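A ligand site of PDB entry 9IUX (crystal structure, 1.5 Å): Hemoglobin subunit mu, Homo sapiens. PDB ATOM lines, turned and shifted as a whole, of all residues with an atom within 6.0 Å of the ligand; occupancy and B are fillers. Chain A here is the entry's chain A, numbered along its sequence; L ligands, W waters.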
ATOM      1  N   LEU A  32     -31.714 -34.858 -11.191  1.00  0.00           N
ATOM      2  CA  LEU A  32     -30.666 -35.484 -11.979  1.00  0.00           C
ATOM      3  C   LEU A  32     -29.925 -36.551 -11.178  1.00  0.00           C
ATOM      4  O   LEU A  32     -29.711 -37.672 -11.659  1.00  0.00           O
ATOM      5  CB  LEU A  32     -29.723 -34.399 -12.494  1.00  0.00           C
ATOM      6  CG  LEU A  32     -28.638 -34.808 -13.492  1.00  0.00           C
ATOM      7  CD1 LEU A  32     -29.220 -35.161 -14.853  1.00  0.00           C
ATOM      8  CD2 LEU A  32     -27.626 -33.672 -13.588  1.00  0.00           C
ATOM      9  N   THR A  39     -24.563 -39.361 -12.585  1.00  0.00           N
ATOM     10  CA  THR A  39     -24.167 -37.963 -12.665  1.00  0.00           C
ATOM     11  C   THR A  39     -23.565 -37.461 -11.355  1.00  0.00           C
ATOM     12  O   THR A  39     -22.930 -36.412 -11.362  1.00  0.00           O
ATOM     13  CB  THR A  39     -25.352 -37.069 -13.042  1.00  0.00           C
ATOM     14  OG1 THR A  39     -26.369 -37.151 -12.032  1.00  0.00           O
ATOM     15  CG2 THR A  39     -25.917 -37.447 -14.413  1.00  0.00           C
ATOM     16  N   TYR A  42     -19.811 -36.098 -10.780  1.00  0.00           N
ATOM     17  CA  TYR A  42     -19.365 -34.764 -11.143  1.00  0.00           C
ATOM     18  C   TYR A  42     -19.476 -33.784  -9.983  1.00  0.00           C
ATOM     19  O   TYR A  42     -18.876 -32.715 -10.036  1.00  0.00           O
ATOM     20  CB  TYR A  42     -20.153 -34.258 -12.352  1.00  0.00           C
ATOM     21  CG  TYR A  42     -19.820 -35.017 -13.606  1.00  0.00           C
ATOM     22  CD1 TYR A  42     -18.644 -34.768 -14.298  1.00  0.00           C
ATOM     23  CD2 TYR A  42     -20.676 -35.990 -14.101  1.00  0.00           C
ATOM     24  CE1 TYR A  42     -18.330 -35.453 -15.449  1.00  0.00           C
ATOM     25  CE2 TYR A  42     -20.367 -36.699 -15.252  1.00  0.00           C
ATOM     26  CZ  TYR A  42     -19.194 -36.420 -15.923  1.00  0.00           C
ATOM     27  OH  TYR A  42     -18.877 -37.105 -17.060  1.00  0.00           O
ATOM     28  N   PHE A  43     -20.214 -34.133  -8.932  1.00  0.00           N
ATOM     29  CA  PHE A  43     -20.499 -33.197  -7.854  1.00  0.00           C
ATOM     30  C   PHE A  43     -20.217 -33.835  -6.499  1.00  0.00           C
ATOM     31  O   PHE A  43     -21.107 -33.955  -5.666  1.00  0.00           O
ATOM     32  CB  PHE A  43     -21.966 -32.741  -7.918  1.00  0.00           C
ATOM     33  CG  PHE A  43     -22.322 -32.029  -9.187  1.00  0.00           C
ATOM     34  CD1 PHE A  43     -22.160 -30.668  -9.300  1.00  0.00           C
ATOM     35  CD2 PHE A  43     -22.840 -32.735 -10.258  1.00  0.00           C
ATOM     36  CE1 PHE A  43     -22.513 -30.013 -10.469  1.00  0.00           C
ATOM     37  CE2 PHE A  43     -23.201 -32.082 -11.434  1.00  0.00           C
ATOM     38  CZ  PHE A  43     -23.032 -30.730 -11.519  1.00  0.00           C
ATOM     39  N   HIS A  45     -18.752 -32.590  -4.041  1.00  0.00           N
ATOM     40  CA  HIS A  45     -18.981 -31.597  -3.004  1.00  0.00           C
ATOM     41  C   HIS A  45     -20.464 -31.489  -2.655  1.00  0.00           C
ATOM     42  O   HIS A  45     -20.815 -31.282  -1.487  1.00  0.00           O
ATOM     43  CB  HIS A  45     -18.408 -30.241  -3.459  1.00  0.00           C
ATOM     44  CG  HIS A  45     -18.796 -29.826  -4.853  1.00  0.00           C
ATOM     45  ND1 HIS A  45     -18.600 -30.625  -5.964  1.00  0.00           N
ATOM     46  CD2 HIS A  45     -19.345 -28.689  -5.317  1.00  0.00           C
ATOM     47  CE1 HIS A  45     -19.017 -29.999  -7.048  1.00  0.00           C
ATOM     48  NE2 HIS A  45     -19.474 -28.818  -6.676  1.00  0.00           N
ATOM     49  N   GLN A  54     -25.298 -25.807  -0.634  1.00  0.00           N
ATOM     50  CA  GLN A  54     -24.391 -25.731  -1.768  1.00  0.00           C
ATOM     51  C   GLN A  54     -25.098 -26.082  -3.067  1.00  0.00           C
ATOM     52  O   GLN A  54     -24.682 -25.622  -4.140  1.00  0.00           O
ATOM     53  CB  GLN A  54     -23.189 -26.644  -1.528  1.00  0.00           C
ATOM     54  CG  GLN A  54     -21.967 -25.950  -0.944  1.00  0.00           C
ATOM     55  CD  GLN A  54     -20.685 -26.689  -1.245  1.00  0.00           C
ATOM     56  OE1 GLN A  54     -20.474 -27.800  -0.766  1.00  0.00           O
ATOM     57  NE2 GLN A  54     -19.830 -26.098  -2.073  1.00  0.00           N
ATOM     58  N   HIS A  58     -24.962 -23.785  -6.523  1.00  0.00           N
ATOM     59  CA  HIS A  58     -24.609 -24.231  -7.862  1.00  0.00           C
ATOM     60  C   HIS A  58     -25.803 -24.113  -8.796  1.00  0.00           C
ATOM     61  O   HIS A  58     -25.636 -23.725  -9.964  1.00  0.00           O
ATOM     62  CB  HIS A  58     -24.110 -25.670  -7.863  1.00  0.00           C
ATOM     63  CG  HIS A  58     -23.606 -26.077  -9.218  1.00  0.00           C
ATOM     64  ND1 HIS A  58     -22.523 -25.460  -9.814  1.00  0.00           N
ATOM     65  CD2 HIS A  58     -24.128 -26.909 -10.154  1.00  0.00           C
ATOM     66  CE1 HIS A  58     -22.352 -25.952 -11.021  1.00  0.00           C
ATOM     67  NE2 HIS A  58     -23.315 -26.839 -11.256  1.00  0.00           N
ATOM     68  N   ARG A  61     -25.946 -20.559 -10.099  1.00  0.00           N
ATOM     69  CA  ARG A  61     -24.945 -20.268 -11.128  1.00  0.00           C
ATOM     70  C   ARG A  61     -25.373 -20.829 -12.471  1.00  0.00           C
ATOM     71  O   ARG A  61     -25.331 -20.152 -13.505  1.00  0.00           O
ATOM     72  CB  ARG A  61     -23.564 -20.856 -10.785  1.00  0.00           C
ATOM     73  CG  ARG A  61     -23.034 -20.525  -9.418  1.00  0.00           C
ATOM     74  CD  ARG A  61     -22.807 -19.031  -9.281  1.00  0.00           C
ATOM     75  NE  ARG A  61     -23.764 -18.461  -8.354  1.00  0.00           N
ATOM     76  CZ  ARG A  61     -23.703 -18.593  -7.031  1.00  0.00           C
ATOM     77  NH1 ARG A  61     -22.684 -19.185  -6.429  1.00  0.00           N
ATOM     78  NH2 ARG A  61     -24.707 -18.151  -6.298  1.00  0.00           N
ATOM     79  N   MHO A  62     -25.773 -22.097 -12.440  1.00  0.00           N
ATOM     80  CA  MHO A  62     -26.116 -22.802 -13.665  1.00  0.00           C
ATOM     81  CB  MHO A  62     -26.452 -24.282 -13.399  1.00  0.00           C
ATOM     82  CG  MHO A  62     -26.651 -25.057 -14.682  1.00  0.00           C
ATOM     83  SD  MHO A  62     -26.911 -26.761 -14.254  1.00  0.00           S
ATOM     84  CE  MHO A  62     -28.397 -26.570 -13.386  1.00  0.00           C
ATOM     85  C   MHO A  62     -27.297 -22.140 -14.377  1.00  0.00           C
ATOM     86  O   MHO A  62     -27.260 -21.856 -15.575  1.00  0.00           O
ATOM     87  OD1 MHO A  62     -25.971 -27.042 -13.138  1.00  0.00           O
ATOM     88  N   LEU A  63     -28.357 -21.839 -13.631  1.00  0.00           N
ATOM     89  CA  LEU A  63     -29.548 -21.279 -14.308  1.00  0.00           C
ATOM     90  C   LEU A  63     -29.342 -19.803 -14.673  1.00  0.00           C
ATOM     91  O   LEU A  63     -29.925 -19.312 -15.655  1.00  0.00           O
ATOM     92  CB  LEU A  63     -30.812 -21.452 -13.449  1.00  0.00           C
ATOM     93  CG  LEU A  63     -31.652 -22.649 -13.841  1.00  0.00           C
ATOM     94  CD1 LEU A  63     -30.828 -23.908 -13.782  1.00  0.00           C
ATOM     95  CD2 LEU A  63     -32.904 -22.783 -13.012  1.00  0.00           C
ATOM     96  N   ALA A  65     -26.580 -18.721 -15.872  1.00  0.00           N
ATOM     97  CA  ALA A  65     -25.898 -18.846 -17.153  1.00  0.00           C
ATOM     98  C   ALA A  65     -26.881 -19.164 -18.259  1.00  0.00           C
ATOM     99  O   ALA A  65     -26.744 -18.672 -19.388  1.00  0.00           O
ATOM    100  CB  ALA A  65     -24.798 -19.911 -17.080  1.00  0.00           C
ATOM    101  N   VAL A  66     -27.915 -19.963 -17.960  1.00  0.00           N
ATOM    102  CA  VAL A  66     -28.945 -20.229 -18.954  1.00  0.00           C
ATOM    103  C   VAL A  66     -29.648 -18.940 -19.352  1.00  0.00           C
ATOM    104  O   VAL A  66     -29.872 -18.674 -20.544  1.00  0.00           O
ATOM    105  CB  VAL A  66     -29.940 -21.272 -18.411  1.00  0.00           C
ATOM    106  CG1 VAL A  66     -31.178 -21.386 -19.341  1.00  0.00           C
ATOM    107  CG2 VAL A  66     -29.272 -22.639 -18.273  1.00  0.00           C
ATOM    108  N   LEU A  83     -17.413 -21.001 -20.736  1.00  0.00           N
ATOM    109  CA  LEU A  83     -18.159 -22.098 -20.141  1.00  0.00           C
ATOM    110  C   LEU A  83     -17.981 -23.380 -20.939  1.00  0.00           C
ATOM    111  O   LEU A  83     -17.995 -24.477 -20.365  1.00  0.00           O
ATOM    112  CB  LEU A  83     -19.629 -21.705 -20.034  1.00  0.00           C
ATOM    113  CG  LEU A  83     -20.496 -22.364 -18.992  1.00  0.00           C
ATOM    114  CD1 LEU A  83     -19.939 -22.109 -17.593  1.00  0.00           C
ATOM    115  CD2 LEU A  83     -21.899 -21.782 -19.134  1.00  0.00           C
ATOM    116  N   LEU A  86     -14.669 -24.711 -19.892  1.00  0.00           N
ATOM    117  CA  LEU A  86     -14.787 -25.291 -18.558  1.00  0.00           C
ATOM    118  C   LEU A  86     -15.386 -26.689 -18.592  1.00  0.00           C
ATOM    119  O   LEU A  86     -14.841 -27.630 -17.998  1.00  0.00           O
ATOM    120  CB  LEU A  86     -15.634 -24.375 -17.663  1.00  0.00           C
ATOM    121  CG  LEU A  86     -15.860 -24.893 -16.247  1.00  0.00           C
ATOM    122  CD1 LEU A  86     -14.563 -24.826 -15.431  1.00  0.00           C
ATOM    123  CD2 LEU A  86     -16.993 -24.123 -15.563  1.00  0.00           C
ATOM    124  N   HIS A  87     -16.521 -26.860 -19.269  1.00  0.00           N
ATOM    125  CA  HIS A  87     -17.200 -28.153 -19.223  1.00  0.00           C
ATOM    126  C   HIS A  87     -16.481 -29.209 -20.055  1.00  0.00           C
ATOM    127  O   HIS A  87     -16.369 -30.357 -19.637  1.00  0.00           O
ATOM    128  CB  HIS A  87     -18.655 -27.999 -19.666  1.00  0.00           C
ATOM    129  CG  HIS A  87     -19.501 -27.369 -18.608  1.00  0.00           C
ATOM    130  ND1 HIS A  87     -19.534 -26.013 -18.415  1.00  0.00           N
ATOM    131  CD2 HIS A  87     -20.321 -27.907 -17.684  1.00  0.00           C
ATOM    132  CE1 HIS A  87     -20.337 -25.730 -17.405  1.00  0.00           C
ATOM    133  NE2 HIS A  87     -20.820 -26.868 -16.938  1.00  0.00           N
ATOM    134  N   LEU A  91     -13.538 -29.699 -16.755  1.00  0.00           N
ATOM    135  CA  LEU A  91     -14.375 -30.624 -16.001  1.00  0.00           C
ATOM    136  C   LEU A  91     -14.509 -31.959 -16.688  1.00  0.00           C
ATOM    137  O   LEU A  91     -14.849 -32.942 -16.022  1.00  0.00           O
ATOM    138  CB  LEU A  91     -15.763 -30.030 -15.803  1.00  0.00           C
ATOM    139  CG  LEU A  91     -15.910 -28.759 -14.973  1.00  0.00           C
ATOM    140  CD1 LEU A  91     -17.292 -28.179 -15.139  1.00  0.00           C
ATOM    141  CD2 LEU A  91     -15.610 -29.029 -13.506  1.00  0.00           C
ATOM    142  N   VAL A  93     -16.845 -33.049 -18.763  1.00  0.00           N
ATOM    143  CA  VAL A  93     -18.204 -33.593 -18.621  1.00  0.00           C
ATOM    144  C   VAL A  93     -18.561 -34.367 -19.880  1.00  0.00           C
ATOM    145  O   VAL A  93     -18.639 -33.789 -20.972  1.00  0.00           O
ATOM    146  CB  VAL A  93     -19.231 -32.484 -18.339  1.00  0.00           C
ATOM    147  CG1 VAL A  93     -20.622 -33.116 -18.187  1.00  0.00           C
ATOM    148  CG2 VAL A  93     -18.857 -31.714 -17.082  1.00  0.00           C
ATOM    149  N   ASN A  97     -24.200 -36.575 -20.642  1.00  0.00           N
ATOM    150  CA  ASN A  97     -24.904 -36.044 -19.486  1.00  0.00           C
ATOM    151  C   ASN A  97     -25.818 -34.883 -19.826  1.00  0.00           C
ATOM    152  O   ASN A  97     -26.765 -34.614 -19.071  1.00  0.00           O
ATOM    153  CB  ASN A  97     -23.910 -35.612 -18.423  1.00  0.00           C
ATOM    154  CG  ASN A  97     -23.174 -36.779 -17.829  1.00  0.00           C
ATOM    155  OD1 ASN A  97     -23.736 -37.521 -17.039  1.00  0.00           O
ATOM    156  ND2 ASN A  97     -21.930 -36.999 -18.267  1.00  0.00           N
ATOM    157  N   PHE A  98     -25.589 -34.215 -20.944  1.00  0.00           N
ATOM    158  CA  PHE A  98     -26.336 -32.983 -21.174  1.00  0.00           C
ATOM    159  C   PHE A  98     -27.812 -33.262 -21.495  1.00  0.00           C
ATOM    160  O   PHE A  98     -28.663 -32.546 -20.969  1.00  0.00           O
ATOM    161  CB  PHE A  98     -25.655 -32.138 -22.253  1.00  0.00           C
ATOM    162  CG  PHE A  98     -24.470 -31.381 -21.714  1.00  0.00           C
ATOM    163  CD1 PHE A  98     -23.268 -32.034 -21.502  1.00  0.00           C
ATOM    164  CD2 PHE A  98     -24.580 -30.041 -21.364  1.00  0.00           C
ATOM    165  CE1 PHE A  98     -22.167 -31.375 -20.955  1.00  0.00           C
ATOM    166  CE2 PHE A  98     -23.480 -29.361 -20.824  1.00  0.00           C
ATOM    167  CZ  PHE A  98     -22.276 -30.023 -20.626  1.00  0.00           C
ATOM    168  N   LEU A 101     -29.632 -33.751 -18.233  1.00  0.00           N
ATOM    169  CA  LEU A 101     -29.931 -32.501 -17.550  1.00  0.00           C
ATOM    170  C   LEU A 101     -31.103 -31.773 -18.207  1.00  0.00           C
ATOM    171  O   LEU A 101     -31.984 -31.260 -17.501  1.00  0.00           O
ATOM    172  CB  LEU A 101     -28.687 -31.599 -17.565  1.00  0.00           C
ATOM    173  CG  LEU A 101     -28.874 -30.250 -16.894  1.00  0.00           C
ATOM    174  CD1 LEU A 101     -29.078 -30.462 -15.409  1.00  0.00           C
ATOM    175  CD2 LEU A 101     -27.674 -29.376 -17.147  1.00  0.00           C
ATOM    176  N   ILE A 102     -31.128 -31.712 -19.541  1.00  0.00           N
ATOM    177  CA  ILE A 102     -32.202 -31.008 -20.236  1.00  0.00           C
ATOM    178  C   ILE A 102     -33.558 -31.654 -19.945  1.00  0.00           C
ATOM    179  O   ILE A 102     -34.528 -30.977 -19.599  1.00  0.00           O
ATOM    180  CB  ILE A 102     -31.909 -30.932 -21.753  1.00  0.00           C
ATOM    181  CG1 ILE A 102     -30.657 -30.070 -21.996  1.00  0.00           C
ATOM    182  CG2 ILE A 102     -33.113 -30.404 -22.541  1.00  0.00           C
ATOM    183  CD1 ILE A 102     -30.140 -30.167 -23.430  1.00  0.00           C
ATOM    184  N   LEU A 129     -32.021 -25.255 -25.471  1.00  0.00           N
ATOM    185  CA  LEU A 129     -31.076 -25.912 -24.584  1.00  0.00           C
ATOM    186  C   LEU A 129     -30.234 -26.945 -25.316  1.00  0.00           C
ATOM    187  O   LEU A 129     -29.064 -27.143 -24.985  1.00  0.00           O
ATOM    188  CB  LEU A 129     -31.809 -26.545 -23.406  1.00  0.00           C
ATOM    189  CG  LEU A 129     -32.390 -25.572 -22.382  1.00  0.00           C
ATOM    190  CD1 LEU A 129     -33.129 -26.375 -21.318  1.00  0.00           C
ATOM    191  CD2 LEU A 129     -31.329 -24.696 -21.752  1.00  0.00           C
ATOM    192  N   VAL A 132     -27.448 -24.940 -26.713  1.00  0.00           N
ATOM    193  CA  VAL A 132     -26.491 -24.609 -25.661  1.00  0.00           C
ATOM    194  C   VAL A 132     -25.603 -25.820 -25.382  1.00  0.00           C
ATOM    195  O   VAL A 132     -24.376 -25.696 -25.248  1.00  0.00           O
ATOM    196  CB  VAL A 132     -27.227 -24.161 -24.388  1.00  0.00           C
ATOM    197  CG1 VAL A 132     -26.292 -24.081 -23.192  1.00  0.00           C
ATOM    198  CG2 VAL A 132     -27.923 -22.801 -24.602  1.00  0.00           C
ATOM    199  N   ALA A 133     -26.215 -27.002 -25.300  1.00  0.00           N
ATOM    200  CA  ALA A 133     -25.449 -28.208 -25.007  1.00  0.00           C
ATOM    201  C   ALA A 133     -24.437 -28.501 -26.110  1.00  0.00           C
ATOM    202  O   ALA A 133     -23.316 -28.932 -25.818  1.00  0.00           O
ATOM    203  CB  ALA A 133     -26.388 -29.407 -24.812  1.00  0.00           C
ATOM    204  N   LEU A 136     -21.497 -26.378 -25.433  1.00  0.00           N
ATOM    205  CA  LEU A 136     -20.755 -26.752 -24.226  1.00  0.00           C
ATOM    206  C   LEU A 136     -20.075 -28.114 -24.337  1.00  0.00           C
ATOM    207  O   LEU A 136     -19.293 -28.459 -23.439  1.00  0.00           O
ATOM    208  CB  LEU A 136     -21.691 -26.757 -23.025  1.00  0.00           C
ATOM    209  CG  LEU A 136     -22.266 -25.376 -22.647  1.00  0.00           C
ATOM    210  CD1 LEU A 136     -23.159 -25.525 -21.437  1.00  0.00           C
ATOM    211  CD2 LEU A 136     -21.186 -24.336 -22.388  1.00  0.00           C
HETATM  212  C1  LIG L   1     -19.957 -25.543 -13.193  1.00  0.00           C
HETATM  213  C2  LIG L   1     -23.430 -23.940 -16.199  1.00  0.00           C
HETATM  214  C3  LIG L   1     -24.308 -28.510 -17.577  1.00  0.00           C
HETATM  215  C4  LIG L   1     -21.217 -30.118 -14.211  1.00  0.00           C
HETATM  216  C5  LIG L   1     -20.808 -24.728 -13.890  1.00  0.00           C
HETATM  217  C6  LIG L   1     -20.833 -23.288 -13.819  1.00  0.00           C
HETATM  218  C7  LIG L   1     -21.798 -22.869 -14.633  1.00  0.00           C
HETATM  219  C8  LIG L   1     -22.407 -24.018 -15.276  1.00  0.00           C
HETATM  220  C9  LIG L   1     -22.208 -21.416 -14.898  1.00  0.00           C
HETATM  221  C10 LIG L   1     -19.919 -22.384 -12.952  1.00  0.00           C
HETATM  222  C11 LIG L   1     -19.967 -22.696 -11.462  1.00  0.00           C
HETATM  223  C12 LIG L   1     -18.924 -21.897 -10.717  1.00  0.00           C
HETATM  224  O1  LIG L   1     -17.942 -21.416 -11.345  1.00  0.00           O
HETATM  225  O2  LIG L   1     -19.094 -21.761  -9.475  1.00  0.00           O
HETATM  226  C13 LIG L   1     -23.939 -25.038 -16.852  1.00  0.00           C
HETATM  227  C14 LIG L   1     -24.933 -25.007 -17.899  1.00  0.00           C
HETATM  228  C15 LIG L   1     -25.189 -26.265 -18.288  1.00  0.00           C
HETATM  229  C16 LIG L   1     -24.359 -27.135 -17.483  1.00  0.00           C
HETATM  230  C17 LIG L   1     -25.538 -23.685 -18.407  1.00  0.00           C
HETATM  231  C18 LIG L   1     -26.167 -26.818 -19.367  1.00  0.00           C
HETATM  232  C19 LIG L   1     -27.105 -26.107 -19.984  1.00  0.00           C
HETATM  233  C20 LIG L   1     -23.588 -29.349 -16.753  1.00  0.00           C
HETATM  234  C21 LIG L   1     -23.683 -30.787 -16.733  1.00  0.00           C
HETATM  235  C22 LIG L   1     -22.813 -31.248 -15.809  1.00  0.00           C
HETATM  236  C23 LIG L   1     -22.171 -30.095 -15.205  1.00  0.00           C
HETATM  237  C24 LIG L   1     -24.612 -31.597 -17.668  1.00  0.00           C
HETATM  238  C25 LIG L   1     -22.519 -32.703 -15.347  1.00  0.00           C
HETATM  239  C26 LIG L   1     -23.448 -33.672 -15.352  1.00  0.00           C
HETATM  240  C27 LIG L   1     -20.614 -29.011 -13.653  1.00  0.00           C
HETATM  241  C28 LIG L   1     -19.607 -29.057 -12.614  1.00  0.00           C
HETATM  242  C29 LIG L   1     -19.253 -27.800 -12.321  1.00  0.00           C
HETATM  243  C30 LIG L   1     -20.019 -26.913 -13.176  1.00  0.00           C
HETATM  244  C31 LIG L   1     -19.085 -30.353 -11.991  1.00  0.00           C
HETATM  245  C32 LIG L   1     -18.213 -27.350 -11.256  1.00  0.00           C
HETATM  246  C33 LIG L   1     -18.943 -27.041  -9.948  1.00  0.00           C
HETATM  247  C34 LIG L   1     -18.041 -26.374  -8.939  1.00  0.00           C
HETATM  248  O3  LIG L   1     -18.542 -25.953  -7.875  1.00  0.00           O
HETATM  249  O4  LIG L   1     -16.820 -26.266  -9.217  1.00  0.00           O
HETATM  250  N1  LIG L   1     -21.780 -25.149 -14.777  1.00  0.00           N
HETATM  251  N2  LIG L   1     -23.597 -26.366 -16.622  1.00  0.00           N
HETATM  252  N3  LIG L   1     -22.665 -28.961 -15.811  1.00  0.00           N
HETATM  253  N4  LIG L   1     -20.844 -27.678 -13.966  1.00  0.00           N
HETATM  254 FE1  LIG L   1     -22.171 -27.042 -15.367  1.00  0.00          FE
HETATM  255  O   HOH W   1     -14.407 -27.635 -10.194  1.00  0.00           O
HETATM  256  O   HOH W   2     -16.127 -19.247 -10.563  1.00  0.00           O
HETATM  257  O   HOH W   3     -14.815 -25.586 -11.745  1.00  0.00           O
HETATM  258  O   HOH W   4     -20.730 -23.660  -8.462  1.00  0.00           O
HETATM  259  O   HOH W   5     -17.100 -22.611  -7.271  1.00  0.00           O
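NE2 of His 87 binds FE1 of the ligand, at 2.1 Å.
NE2 of His 45 sits at hydrogen-bond distance from O3 of the ligand, at 3.2 Å.
A ring nitrogen (NE2) of His 58 sits at hydrogen-bond distance from OD1 of MHO 62, at 3.3 Å.
O of His 87 lies within hydrogen-bond range of N of Val 93.
The backbone carbonyl oxygen (O) of Leu 86 lies within hydrogen-bond range of the backbone NH (N) of Leu 91.
The side-chain hydroxyl (OH) of Tyr 42 sits at hydrogen-bond distance from the side-chain amide nitrogen (ND2) of Asn 97.
A ring nitrogen (ND1) of His 87 sits at hydrogen-bond distance from the backbone carbonyl oxygen (O) of Leu 83 (2.9 Å).
Merely in contact with the ligand: Tyr 42, Phe 43, His 58, Arg 61, MHO 62, Ala 65, Val 66, Leu 83, Leu 91, Val 93, Asn 97, Phe 98, Leu 101, Val 132 and Leu 136.
Hydrophobic or aromatic side chains within 4 Å of the ligand: Tyr 42, Phe 43, His 45, His 58, Ala 65, Val 66, Leu 83, His 87, Leu 91, Val 93, Phe 98, Leu 101, Val 132 and Leu 136.
Of the 25 residues printed, 17 come within 4 Å of the ligand.
Along chain A the residues within 4 Å of the ligand span positions 42 to 136.
The nearest printed residue that does not touch the ligand is Leu 86 (4.1 Å).
Water W4 lies within hydrogen-bond range of O2 of the ligand (2.7 Å) and ND1 of His 58 (2.9 Å).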
